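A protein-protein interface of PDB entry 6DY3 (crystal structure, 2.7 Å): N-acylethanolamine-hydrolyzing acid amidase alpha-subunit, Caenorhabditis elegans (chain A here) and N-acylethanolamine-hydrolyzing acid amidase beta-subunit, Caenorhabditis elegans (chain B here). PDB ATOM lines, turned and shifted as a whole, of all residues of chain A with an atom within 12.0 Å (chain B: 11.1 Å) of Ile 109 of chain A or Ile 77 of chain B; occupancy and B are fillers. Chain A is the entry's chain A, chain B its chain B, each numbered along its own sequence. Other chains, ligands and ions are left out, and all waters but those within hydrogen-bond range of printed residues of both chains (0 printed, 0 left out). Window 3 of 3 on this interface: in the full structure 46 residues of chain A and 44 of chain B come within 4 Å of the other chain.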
ATOM      1  N   LYS A  49     -15.394  24.794  17.626  1.00  0.00           N
ATOM      2  CA  LYS A  49     -16.430  24.962  18.635  1.00  0.00           C
ATOM      3  C   LYS A  49     -17.794  25.257  18.027  1.00  0.00           C
ATOM      4  O   LYS A  49     -18.813  25.052  18.694  1.00  0.00           O
ATOM      5  CB  LYS A  49     -16.025  26.087  19.581  1.00  0.00           C
ATOM      6  CG  LYS A  49     -14.735  25.812  20.326  1.00  0.00           C
ATOM      7  CD  LYS A  49     -14.376  26.961  21.246  1.00  0.00           C
ATOM      8  CE  LYS A  49     -13.024  26.742  21.906  1.00  0.00           C
ATOM      9  NZ  LYS A  49     -12.622  27.904  22.752  1.00  0.00           N
ATOM     10  N   TYR A  50     -17.843  25.738  16.784  1.00  0.00           N
ATOM     11  CA  TYR A  50     -19.115  26.039  16.143  1.00  0.00           C
ATOM     12  C   TYR A  50     -19.779  24.812  15.537  1.00  0.00           C
ATOM     13  O   TYR A  50     -20.963  24.878  15.191  1.00  0.00           O
ATOM     14  CB  TYR A  50     -18.917  27.093  15.056  1.00  0.00           C
ATOM     15  CG  TYR A  50     -18.696  28.495  15.589  1.00  0.00           C
ATOM     16  CD1 TYR A  50     -19.750  29.390  15.708  1.00  0.00           C
ATOM     17  CD2 TYR A  50     -17.427  28.922  15.968  1.00  0.00           C
ATOM     18  CE1 TYR A  50     -19.547  30.675  16.186  1.00  0.00           C
ATOM     19  CE2 TYR A  50     -17.214  30.205  16.447  1.00  0.00           C
ATOM     20  CZ  TYR A  50     -18.276  31.077  16.553  1.00  0.00           C
ATOM     21  OH  TYR A  50     -18.067  32.352  17.027  1.00  0.00           O
ATOM     22  N   ILE A  51     -19.049  23.715  15.379  1.00  0.00           N
ATOM     23  CA  ILE A  51     -19.639  22.481  14.853  1.00  0.00           C
ATOM     24  C   ILE A  51     -20.468  21.830  15.956  1.00  0.00           C
ATOM     25  O   ILE A  51     -19.957  21.651  17.074  1.00  0.00           O
ATOM     26  CB  ILE A  51     -18.551  21.529  14.356  1.00  0.00           C
ATOM     27  CG1 ILE A  51     -17.628  22.227  13.353  1.00  0.00           C
ATOM     28  CG2 ILE A  51     -19.185  20.304  13.702  1.00  0.00           C
ATOM     29  CD1 ILE A  51     -16.453  21.383  12.890  1.00  0.00           C
ATOM     30  N   PRO A  52     -21.726  21.464  15.697  1.00  0.00           N
ATOM     31  CA  PRO A  52     -22.522  20.789  16.734  1.00  0.00           C
ATOM     32  C   PRO A  52     -21.810  19.550  17.253  1.00  0.00           C
ATOM     33  O   PRO A  52     -21.343  18.713  16.479  1.00  0.00           O
ATOM     34  CB  PRO A  52     -23.823  20.432  16.007  1.00  0.00           C
ATOM     35  CG  PRO A  52     -23.908  21.397  14.884  1.00  0.00           C
ATOM     36  CD  PRO A  52     -22.497  21.662  14.458  1.00  0.00           C
ATOM     37  N   LYS A  53     -21.738  19.433  18.579  1.00  0.00           N
ATOM     38  CA  LYS A  53     -20.961  18.353  19.180  1.00  0.00           C
ATOM     39  C   LYS A  53     -21.414  16.968  18.733  1.00  0.00           C
ATOM     40  O   LYS A  53     -20.541  16.113  18.501  1.00  0.00           O
ATOM     41  CB  LYS A  53     -21.009  18.468  20.708  1.00  0.00           C
ATOM     42  CG  LYS A  53     -20.037  17.539  21.418  1.00  0.00           C
ATOM     43  CD  LYS A  53     -19.909  17.879  22.896  1.00  0.00           C
ATOM     44  CE  LYS A  53     -18.886  16.989  23.586  1.00  0.00           C
ATOM     45  NZ  LYS A  53     -18.570  17.457  24.969  1.00  0.00           N
ATOM     46  N   PRO A  54     -22.712  16.672  18.599  1.00  0.00           N
ATOM     47  CA  PRO A  54     -23.102  15.326  18.146  1.00  0.00           C
ATOM     48  C   PRO A  54     -22.547  14.962  16.776  1.00  0.00           C
ATOM     49  O   PRO A  54     -22.348  13.772  16.493  1.00  0.00           O
ATOM     50  CB  PRO A  54     -24.637  15.390  18.139  1.00  0.00           C
ATOM     51  CG  PRO A  54     -24.978  16.477  19.099  1.00  0.00           C
ATOM     52  CD  PRO A  54     -23.883  17.491  18.955  1.00  0.00           C
ATOM     53  N   LEU A  55     -22.293  15.946  15.914  1.00  0.00           N
ATOM     54  CA  LEU A  55     -21.804  15.680  14.567  1.00  0.00           C
ATOM     55  C   LEU A  55     -20.296  15.819  14.434  1.00  0.00           C
ATOM     56  O   LEU A  55     -19.757  15.544  13.359  1.00  0.00           O
ATOM     57  CB  LEU A  55     -22.496  16.601  13.554  1.00  0.00           C
ATOM     58  CG  LEU A  55     -23.952  16.259  13.221  1.00  0.00           C
ATOM     59  CD1 LEU A  55     -24.505  17.257  12.245  1.00  0.00           C
ATOM     60  CD2 LEU A  55     -24.085  14.858  12.647  1.00  0.00           C
ATOM     61  N   VAL A 101     -19.743  27.344   8.927  1.00  0.00           N
ATOM     62  CA  VAL A 101     -20.092  26.800  10.233  1.00  0.00           C
ATOM     63  C   VAL A 101     -19.887  27.841  11.325  1.00  0.00           C
ATOM     64  O   VAL A 101     -20.641  27.877  12.306  1.00  0.00           O
ATOM     65  CB  VAL A 101     -19.285  25.519  10.511  1.00  0.00           C
ATOM     66  CG1 VAL A 101     -17.799  25.828  10.674  1.00  0.00           C
ATOM     67  CG2 VAL A 101     -19.833  24.808  11.726  1.00  0.00           C
ATOM     68  N   PHE A 104     -22.533  31.799  11.229  1.00  0.00           N
ATOM     69  CA  PHE A 104     -23.823  32.033  11.864  1.00  0.00           C
ATOM     70  C   PHE A 104     -23.934  31.093  13.057  1.00  0.00           C
ATOM     71  O   PHE A 104     -23.991  29.873  12.885  1.00  0.00           O
ATOM     72  CB  PHE A 104     -24.961  31.812  10.863  1.00  0.00           C
ATOM     73  CG  PHE A 104     -26.313  32.205  11.379  1.00  0.00           C
ATOM     74  CD1 PHE A 104     -26.535  33.476  11.877  1.00  0.00           C
ATOM     75  CD2 PHE A 104     -27.366  31.308  11.354  1.00  0.00           C
ATOM     76  CE1 PHE A 104     -27.785  33.843  12.352  1.00  0.00           C
ATOM     77  CE2 PHE A 104     -28.617  31.669  11.827  1.00  0.00           C
ATOM     78  CZ  PHE A 104     -28.826  32.936  12.325  1.00  0.00           C
ATOM     79  N   ASP A 105     -23.950  31.656  14.262  1.00  0.00           N
ATOM     80  CA  ASP A 105     -23.943  30.843  15.474  1.00  0.00           C
ATOM     81  C   ASP A 105     -25.288  30.147  15.652  1.00  0.00           C
ATOM     82  O   ASP A 105     -26.322  30.806  15.809  1.00  0.00           O
ATOM     83  CB  ASP A 105     -23.627  31.713  16.687  1.00  0.00           C
ATOM     84  CG  ASP A 105     -23.121  30.907  17.868  1.00  0.00           C
ATOM     85  OD1 ASP A 105     -23.300  29.672  17.871  1.00  0.00           O
ATOM     86  OD2 ASP A 105     -22.535  31.511  18.791  1.00  0.00           O
ATOM     87  N   ARG A 106     -25.270  28.814  15.639  1.00  0.00           N
ATOM     88  CA  ARG A 106     -26.480  28.010  15.764  1.00  0.00           C
ATOM     89  C   ARG A 106     -26.336  26.965  16.866  1.00  0.00           C
ATOM     90  O   ARG A 106     -26.999  25.924  16.837  1.00  0.00           O
ATOM     91  CB  ARG A 106     -26.825  27.346  14.430  1.00  0.00           C
ATOM     92  CG  ARG A 106     -27.331  28.323  13.383  1.00  0.00           C
ATOM     93  CD  ARG A 106     -27.520  27.664  12.025  1.00  0.00           C
ATOM     94  NE  ARG A 106     -26.248  27.395  11.355  1.00  0.00           N
ATOM     95  CZ  ARG A 106     -26.136  26.998  10.089  1.00  0.00           C
ATOM     96  NH1 ARG A 106     -27.225  26.826   9.345  1.00  0.00           N
ATOM     97  NH2 ARG A 106     -24.934  26.777   9.563  1.00  0.00           N
ATOM     98  N   ARG A 107     -25.481  27.233  17.855  1.00  0.00           N
ATOM     99  CA  ARG A 107     -25.263  26.279  18.933  1.00  0.00           C
ATOM    100  C   ARG A 107     -26.404  26.274  19.943  1.00  0.00           C
ATOM    101  O   ARG A 107     -26.629  25.259  20.612  1.00  0.00           O
ATOM    102  CB  ARG A 107     -23.941  26.585  19.636  1.00  0.00           C
ATOM    103  CG  ARG A 107     -22.715  26.234  18.811  1.00  0.00           C
ATOM    104  CD  ARG A 107     -21.435  26.770  19.442  1.00  0.00           C
ATOM    105  NE  ARG A 107     -21.367  28.227  19.408  1.00  0.00           N
ATOM    106  CZ  ARG A 107     -20.314  28.934  19.806  1.00  0.00           C
ATOM    107  NH1 ARG A 107     -19.237  28.319  20.273  1.00  0.00           N
ATOM    108  NH2 ARG A 107     -20.336  30.260  19.733  1.00  0.00           N
ATOM    109  N   HIS A 108     -27.131  27.387  20.071  1.00  0.00           N
ATOM    110  CA  HIS A 108     -28.283  27.426  20.965  1.00  0.00           C
ATOM    111  C   HIS A 108     -29.348  26.410  20.571  1.00  0.00           C
ATOM    112  O   HIS A 108     -30.149  26.007  21.421  1.00  0.00           O
ATOM    113  CB  HIS A 108     -28.886  28.830  20.977  1.00  0.00           C
ATOM    114  CG  HIS A 108     -29.396  29.277  19.641  1.00  0.00           C
ATOM    115  ND1 HIS A 108     -28.560  29.687  18.624  1.00  0.00           N
ATOM    116  CD2 HIS A 108     -30.655  29.377  19.154  1.00  0.00           C
ATOM    117  CE1 HIS A 108     -29.281  30.021  17.570  1.00  0.00           C
ATOM    118  NE2 HIS A 108     -30.557  29.842  17.865  1.00  0.00           N
ATOM    119  N   ILE A 109     -29.376  25.989  19.303  1.00  0.00           N
ATOM    120  CA  ILE A 109     -30.350  24.994  18.864  1.00  0.00           C
ATOM    121  C   ILE A 109     -30.029  23.630  19.456  1.00  0.00           C
ATOM    122  O   ILE A 109     -30.936  22.828  19.710  1.00  0.00           O
ATOM    123  CB  ILE A 109     -30.397  24.942  17.323  1.00  0.00           C
ATOM    124  CG1 ILE A 109     -30.707  26.328  16.742  1.00  0.00           C
ATOM    125  CG2 ILE A 109     -31.426  23.922  16.851  1.00  0.00           C
ATOM    126  CD1 ILE A 109     -32.033  26.921  17.197  1.00  0.00           C
ATOM    127  N   PHE A 110     -28.752  23.336  19.679  1.00  0.00           N
ATOM    128  CA  PHE A 110     -28.346  22.077  20.297  1.00  0.00           C
ATOM    129  C   PHE A 110     -28.177  22.236  21.807  1.00  0.00           C
ATOM    130  O   PHE A 110     -28.877  21.597  22.593  1.00  0.00           O
ATOM    131  CB  PHE A 110     -27.043  21.576  19.675  1.00  0.00           C
ATOM    132  CG  PHE A 110     -27.180  21.162  18.240  1.00  0.00           C
ATOM    133  CD1 PHE A 110     -27.290  19.822  17.902  1.00  0.00           C
ATOM    134  CD2 PHE A 110     -27.206  22.111  17.228  1.00  0.00           C
ATOM    135  CE1 PHE A 110     -27.416  19.437  16.584  1.00  0.00           C
ATOM    136  CE2 PHE A 110     -27.336  21.730  15.906  1.00  0.00           C
ATOM    137  CZ  PHE A 110     -27.442  20.393  15.587  1.00  0.00           C
ATOM    138  N   TYR B  72     -30.132  30.451   5.256  1.00  0.00           N
ATOM    139  CA  TYR B  72     -30.593  29.797   6.473  1.00  0.00           C
ATOM    140  C   TYR B  72     -32.110  29.851   6.522  1.00  0.00           C
ATOM    141  O   TYR B  72     -32.699  30.936   6.572  1.00  0.00           O
ATOM    142  CB  TYR B  72     -29.998  30.458   7.721  1.00  0.00           C
ATOM    143  CG  TYR B  72     -28.497  30.593   7.681  1.00  0.00           C
ATOM    144  CD1 TYR B  72     -27.682  29.468   7.719  1.00  0.00           C
ATOM    145  CD2 TYR B  72     -27.891  31.846   7.624  1.00  0.00           C
ATOM    146  CE1 TYR B  72     -26.304  29.581   7.687  1.00  0.00           C
ATOM    147  CE2 TYR B  72     -26.514  31.973   7.596  1.00  0.00           C
ATOM    148  CZ  TYR B  72     -25.722  30.833   7.628  1.00  0.00           C
ATOM    149  OH  TYR B  72     -24.348  30.936   7.597  1.00  0.00           O
ATOM    150  N   SER B  73     -32.732  28.684   6.531  1.00  0.00           N
ATOM    151  CA  SER B  73     -34.171  28.563   6.676  1.00  0.00           C
ATOM    152  C   SER B  73     -34.455  27.893   8.016  1.00  0.00           C
ATOM    153  O   SER B  73     -33.538  27.544   8.769  1.00  0.00           O
ATOM    154  CB  SER B  73     -34.764  27.767   5.509  1.00  0.00           C
ATOM    155  OG  SER B  73     -34.457  28.371   4.259  1.00  0.00           O
ATOM    156  N   GLY B  74     -35.731  27.730   8.325  1.00  0.00           N
ATOM    157  CA  GLY B  74     -36.115  27.076   9.553  1.00  0.00           C
ATOM    158  C   GLY B  74     -35.780  25.596   9.519  1.00  0.00           C
ATOM    159  O   GLY B  74     -35.204  25.065   8.569  1.00  0.00           O
ATOM    160  N   ALA B  75     -36.151  24.918  10.603  1.00  0.00           N
ATOM    161  CA  ALA B  75     -36.034  23.463  10.683  1.00  0.00           C
ATOM    162  C   ALA B  75     -34.587  23.016  10.512  1.00  0.00           C
ATOM    163  O   ALA B  75     -34.292  22.046   9.810  1.00  0.00           O
ATOM    164  CB  ALA B  75     -36.941  22.790   9.651  1.00  0.00           C
ATOM    165  N   TYR B  76     -33.671  23.738  11.160  1.00  0.00           N
ATOM    166  CA  TYR B  76     -32.265  23.352  11.134  1.00  0.00           C
ATOM    167  C   TYR B  76     -32.070  21.965  11.732  1.00  0.00           C
ATOM    168  O   TYR B  76     -31.219  21.196  11.271  1.00  0.00           O
ATOM    169  CB  TYR B  76     -31.441  24.393  11.890  1.00  0.00           C
ATOM    170  CG  TYR B  76     -29.947  24.253  11.735  1.00  0.00           C
ATOM    171  CD1 TYR B  76     -29.353  24.273  10.478  1.00  0.00           C
ATOM    172  CD2 TYR B  76     -29.125  24.131  12.850  1.00  0.00           C
ATOM    173  CE1 TYR B  76     -27.982  24.152  10.331  1.00  0.00           C
ATOM    174  CE2 TYR B  76     -27.751  24.014  12.715  1.00  0.00           C
ATOM    175  CZ  TYR B  76     -27.184  24.024  11.450  1.00  0.00           C
ATOM    176  OH  TYR B  76     -25.818  23.912  11.297  1.00  0.00           O
ATOM    177  N   ILE B  77     -32.855  21.625  12.757  1.00  0.00           N
ATOM    178  CA  ILE B  77     -32.800  20.282  13.330  1.00  0.00           C
ATOM    179  C   ILE B  77     -33.229  19.251  12.296  1.00  0.00           C
ATOM    180  O   ILE B  77     -32.556  18.234  12.090  1.00  0.00           O
ATOM    181  CB  ILE B  77     -33.679  20.204  14.592  1.00  0.00           C
ATOM    182  CG1 ILE B  77     -33.063  21.043  15.717  1.00  0.00           C
ATOM    183  CG2 ILE B  77     -33.875  18.748  15.038  1.00  0.00           C
ATOM    184  CD1 ILE B  77     -33.945  21.174  16.945  1.00  0.00           C
ATOM    185  N   ASP B  78     -34.367  19.492  11.638  1.00  0.00           N
ATOM    186  CA  ASP B  78     -34.925  18.498  10.726  1.00  0.00           C
ATOM    187  C   ASP B  78     -33.984  18.206   9.570  1.00  0.00           C
ATOM    188  O   ASP B  78     -33.975  17.085   9.051  1.00  0.00           O
ATOM    189  CB  ASP B  78     -36.266  18.972  10.171  1.00  0.00           C
ATOM    190  CG  ASP B  78     -37.384  18.902  11.194  1.00  0.00           C
ATOM    191  OD1 ASP B  78     -37.075  18.844  12.404  1.00  0.00           O
ATOM    192  OD2 ASP B  78     -38.567  18.907  10.792  1.00  0.00           O
ATOM    193  N   ASN B  79     -33.192  19.194   9.155  1.00  0.00           N
ATOM    194  CA  ASN B  79     -32.464  19.117   7.897  1.00  0.00           C
ATOM    195  C   ASN B  79     -30.951  19.136   8.040  1.00  0.00           C
ATOM    196  O   ASN B  79     -30.258  19.205   7.010  1.00  0.00           O
ATOM    197  CB  ASN B  79     -32.884  20.273   6.980  1.00  0.00           C
ATOM    198  CG  ASN B  79     -34.342  20.221   6.598  1.00  0.00           C
ATOM    199  OD1 ASN B  79     -35.007  21.254   6.574  1.00  0.00           O
ATOM    200  ND2 ASN B  79     -34.850  19.025   6.294  1.00  0.00           N
ATOM    201  N   ILE B  80     -30.417  19.042   9.253  1.00  0.00           N
ATOM    202  CA  ILE B  80     -28.975  19.195   9.441  1.00  0.00           C
ATOM    203  C   ILE B  80     -28.215  18.133   8.656  1.00  0.00           C
ATOM    204  O   ILE B  80     -27.184  18.415   8.041  1.00  0.00           O
ATOM    205  CB  ILE B  80     -28.617  19.148  10.942  1.00  0.00           C
ATOM    206  CG1 ILE B  80     -27.107  19.258  11.079  1.00  0.00           C
ATOM    207  CG2 ILE B  80     -29.118  17.851  11.610  1.00  0.00           C
ATOM    208  CD1 ILE B  80     -26.656  19.743  12.417  1.00  0.00           C
ATOM    209  N   LEU B  81     -28.725  16.894   8.656  1.00  0.00           N
ATOM    210  CA  LEU B  81     -28.075  15.810   7.930  1.00  0.00           C
ATOM    211  C   LEU B  81     -28.041  16.100   6.441  1.00  0.00           C
ATOM    212  O   LEU B  81     -27.020  15.867   5.777  1.00  0.00           O
ATOM    213  CB  LEU B  81     -28.799  14.491   8.178  1.00  0.00           C
ATOM    214  CG  LEU B  81     -28.629  13.876   9.563  1.00  0.00           C
ATOM    215  CD1 LEU B  81     -29.259  12.505   9.546  1.00  0.00           C
ATOM    216  CD2 LEU B  81     -27.180  13.799  10.000  1.00  0.00           C
ATOM    217  N   MET B  82     -29.154  16.589   5.892  1.00  0.00           N
ATOM    218  CA  MET B  82     -29.195  16.932   4.477  1.00  0.00           C
ATOM    219  C   MET B  82     -28.310  18.136   4.167  1.00  0.00           C
ATOM    220  O   MET B  82     -27.742  18.215   3.072  1.00  0.00           O
ATOM    221  CB  MET B  82     -30.648  17.207   4.056  1.00  0.00           C
ATOM    222  CG  MET B  82     -30.882  17.283   2.567  1.00  0.00           C
ATOM    223  SD  MET B  82     -30.378  15.782   1.708  1.00  0.00           S
ATOM    224  CE  MET B  82     -30.684  16.247  -0.001  1.00  0.00           C
ATOM    225  N   GLU B  83     -28.174  19.080   5.105  1.00  0.00           N
ATOM    226  CA  GLU B  83     -27.260  20.202   4.908  1.00  0.00           C
ATOM    227  C   GLU B  83     -25.819  19.715   4.822  1.00  0.00           C
ATOM    228  O   GLU B  83     -25.080  20.074   3.899  1.00  0.00           O
ATOM    229  CB  GLU B  83     -27.409  21.219   6.048  1.00  0.00           C
ATOM    230  CG  GLU B  83     -28.787  21.887   6.149  1.00  0.00           C
ATOM    231  CD  GLU B  83     -28.934  23.135   5.281  1.00  0.00           C
ATOM    232  OE1 GLU B  83     -27.976  23.496   4.560  1.00  0.00           O
ATOM    233  OE2 GLU B  83     -30.017  23.764   5.323  1.00  0.00           O
ATOM    234  N   PHE B  84     -25.399  18.900   5.791  1.00  0.00           N
ATOM    235  CA  PHE B  84     -24.049  18.347   5.760  1.00  0.00           C
ATOM    236  C   PHE B  84     -23.835  17.474   4.532  1.00  0.00           C
ATOM    237  O   PHE B  84     -22.736  17.444   3.969  1.00  0.00           O
ATOM    238  CB  PHE B  84     -23.786  17.543   7.032  1.00  0.00           C
ATOM    239  CG  PHE B  84     -23.322  18.375   8.194  1.00  0.00           C
ATOM    240  CD1 PHE B  84     -22.245  17.965   8.969  1.00  0.00           C
ATOM    241  CD2 PHE B  84     -23.961  19.563   8.514  1.00  0.00           C
ATOM    242  CE1 PHE B  84     -21.813  18.726  10.044  1.00  0.00           C
ATOM    243  CE2 PHE B  84     -23.532  20.333   9.589  1.00  0.00           C
ATOM    244  CZ  PHE B  84     -22.457  19.914  10.355  1.00  0.00           C
ATOM    245  N   ARG B 141     -33.533  24.072  -1.701  1.00  0.00           N
ATOM    246  CA  ARG B 141     -33.459  22.726  -1.163  1.00  0.00           C
ATOM    247  C   ARG B 141     -34.002  21.740  -2.212  1.00  0.00           C
ATOM    248  O   ARG B 141     -35.201  21.789  -2.518  1.00  0.00           O
ATOM    249  CB  ARG B 141     -34.258  22.615   0.128  1.00  0.00           C
ATOM    250  CG  ARG B 141     -33.651  23.381   1.285  1.00  0.00           C
ATOM    251  CD  ARG B 141     -34.556  23.336   2.498  1.00  0.00           C
ATOM    252  NE  ARG B 141     -33.901  23.852   3.697  1.00  0.00           N
ATOM    253  CZ  ARG B 141     -34.516  24.035   4.865  1.00  0.00           C
ATOM    254  NH1 ARG B 141     -35.807  23.749   4.990  1.00  0.00           N
ATOM    255  NH2 ARG B 141     -33.838  24.504   5.910  1.00  0.00           N
ATOM    256  N   TRP B 142     -33.172  20.852  -2.774  1.00  0.00           N
ATOM    257  CA  TRP B 142     -31.726  20.740  -2.512  1.00  0.00           C
ATOM    258  C   TRP B 142     -30.949  20.660  -3.813  1.00  0.00           C
ATOM    259  O   TRP B 142     -29.738  20.444  -3.799  1.00  0.00           O
ATOM    260  CB  TRP B 142     -31.437  19.506  -1.656  1.00  0.00           C
ATOM    261  CG  TRP B 142     -32.085  19.548  -0.303  1.00  0.00           C
ATOM    262  CD1 TRP B 142     -33.289  19.016   0.045  1.00  0.00           C
ATOM    263  CD2 TRP B 142     -31.555  20.150   0.886  1.00  0.00           C
ATOM    264  NE1 TRP B 142     -33.547  19.253   1.372  1.00  0.00           N
ATOM    265  CE2 TRP B 142     -32.499  19.949   1.911  1.00  0.00           C
ATOM    266  CE3 TRP B 142     -30.376  20.839   1.180  1.00  0.00           C
ATOM    267  CZ2 TRP B 142     -32.299  20.409   3.212  1.00  0.00           C
ATOM    268  CZ3 TRP B 142     -30.181  21.298   2.469  1.00  0.00           C
ATOM    269  CH2 TRP B 142     -31.138  21.081   3.470  1.00  0.00           C
ATOM    270  N   LYS B 168     -38.417  36.183   7.625  1.00  0.00           N
ATOM    271  CA  LYS B 168     -37.147  36.654   8.167  1.00  0.00           C
ATOM    272  C   LYS B 168     -36.401  37.515   7.157  1.00  0.00           C
ATOM    273  O   LYS B 168     -35.701  38.456   7.544  1.00  0.00           O
ATOM    274  CB  LYS B 168     -36.289  35.464   8.603  1.00  0.00           C
ATOM    275  CG  LYS B 168     -35.022  35.855   9.349  1.00  0.00           C
ATOM    276  CD  LYS B 168     -35.335  36.286  10.768  1.00  0.00           C
ATOM    277  CE  LYS B 168     -34.090  36.758  11.511  1.00  0.00           C
ATOM    278  NZ  LYS B 168     -33.100  35.665  11.717  1.00  0.00           N
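NH2 of Arg 106 of chain A sits close to OH of Tyr 76 of chain B, at 3.5 Å.
Printed residues of chain A that touch a printed residue of chain B: Leu 55, Phe 104, Arg 106, Ile 109 and Phe 110.
Hydrophobic or aromatic side chains of chain A that line the printed part of chain B: Leu 55, Phe 104, Ile 109 and Phe 110.
Of the 16 printed residues of chain B, 5 touch a printed residue of chain A.
Printed residues of chain B that touch a printed residue of chain A: Tyr 72, Tyr 76, Ile 77, Ile 80 and Phe 84.
Hydrophobic or aromatic side chains of chain B that line the printed part of chain A: Tyr 72, Tyr 76, Ile 77, Ile 80 and Phe 84.
Along chain B the printed residues that touch a printed residue of chain A span positions 72 to 84.
Among the printed residues, no Asp or Glu carboxylate lies within 4 Å of a Lys or Arg side-chain nitrogen of the other chain.
Among the printed residues, pairs that only touch across the chains: Arg 106 of chain A with Tyr 72 of chain B (3.1 Å), Leu 55 of chain A with Ile 80 of chain B (3.3 Å), Phe 110 of chain A with Ile 80 of chain B (3.3 Å), Phe 104 of chain A with Tyr 72 of chain B (3.4 Å), Ile 109 of chain A with Ile 77 of chain B (3.5 Å), Leu 55 of chain A with Phe 84 of chain B (3.8 Å) and Phe 110 of chain A with Tyr 76 of chain B (3.9 Å).
Printed residues of chain B within 4 Å of Leu 55 of chain A: Ile 80 and Phe 84.
Of chain B, only Ile 77 (3.5 Å) comes within 4 Å of Ile 109 of chain A.
Phe 110 of chain A touches two residues of chain B.
Tyr 76 of chain B touches two residues of chain A.
Of chain A, only Ile 109 comes within 4 Å of Ile 77 of chain B.
No residue of chain A comes within 4 Å of Asp 78 of chain B.
No residue of chain A comes within 4 Å of Asn 79 of chain B.
Ile 80 of chain B touches just these residues of chain A: Leu 55 and Phe 110.
Printed residues of chain A within 4 Å of Phe 84 of chain B: Leu 55 (3.8 Å).
The nearest printed residue of chain B that does not touch Phe 104 of chain A is Lys 168 of chain B (5.1 Å).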
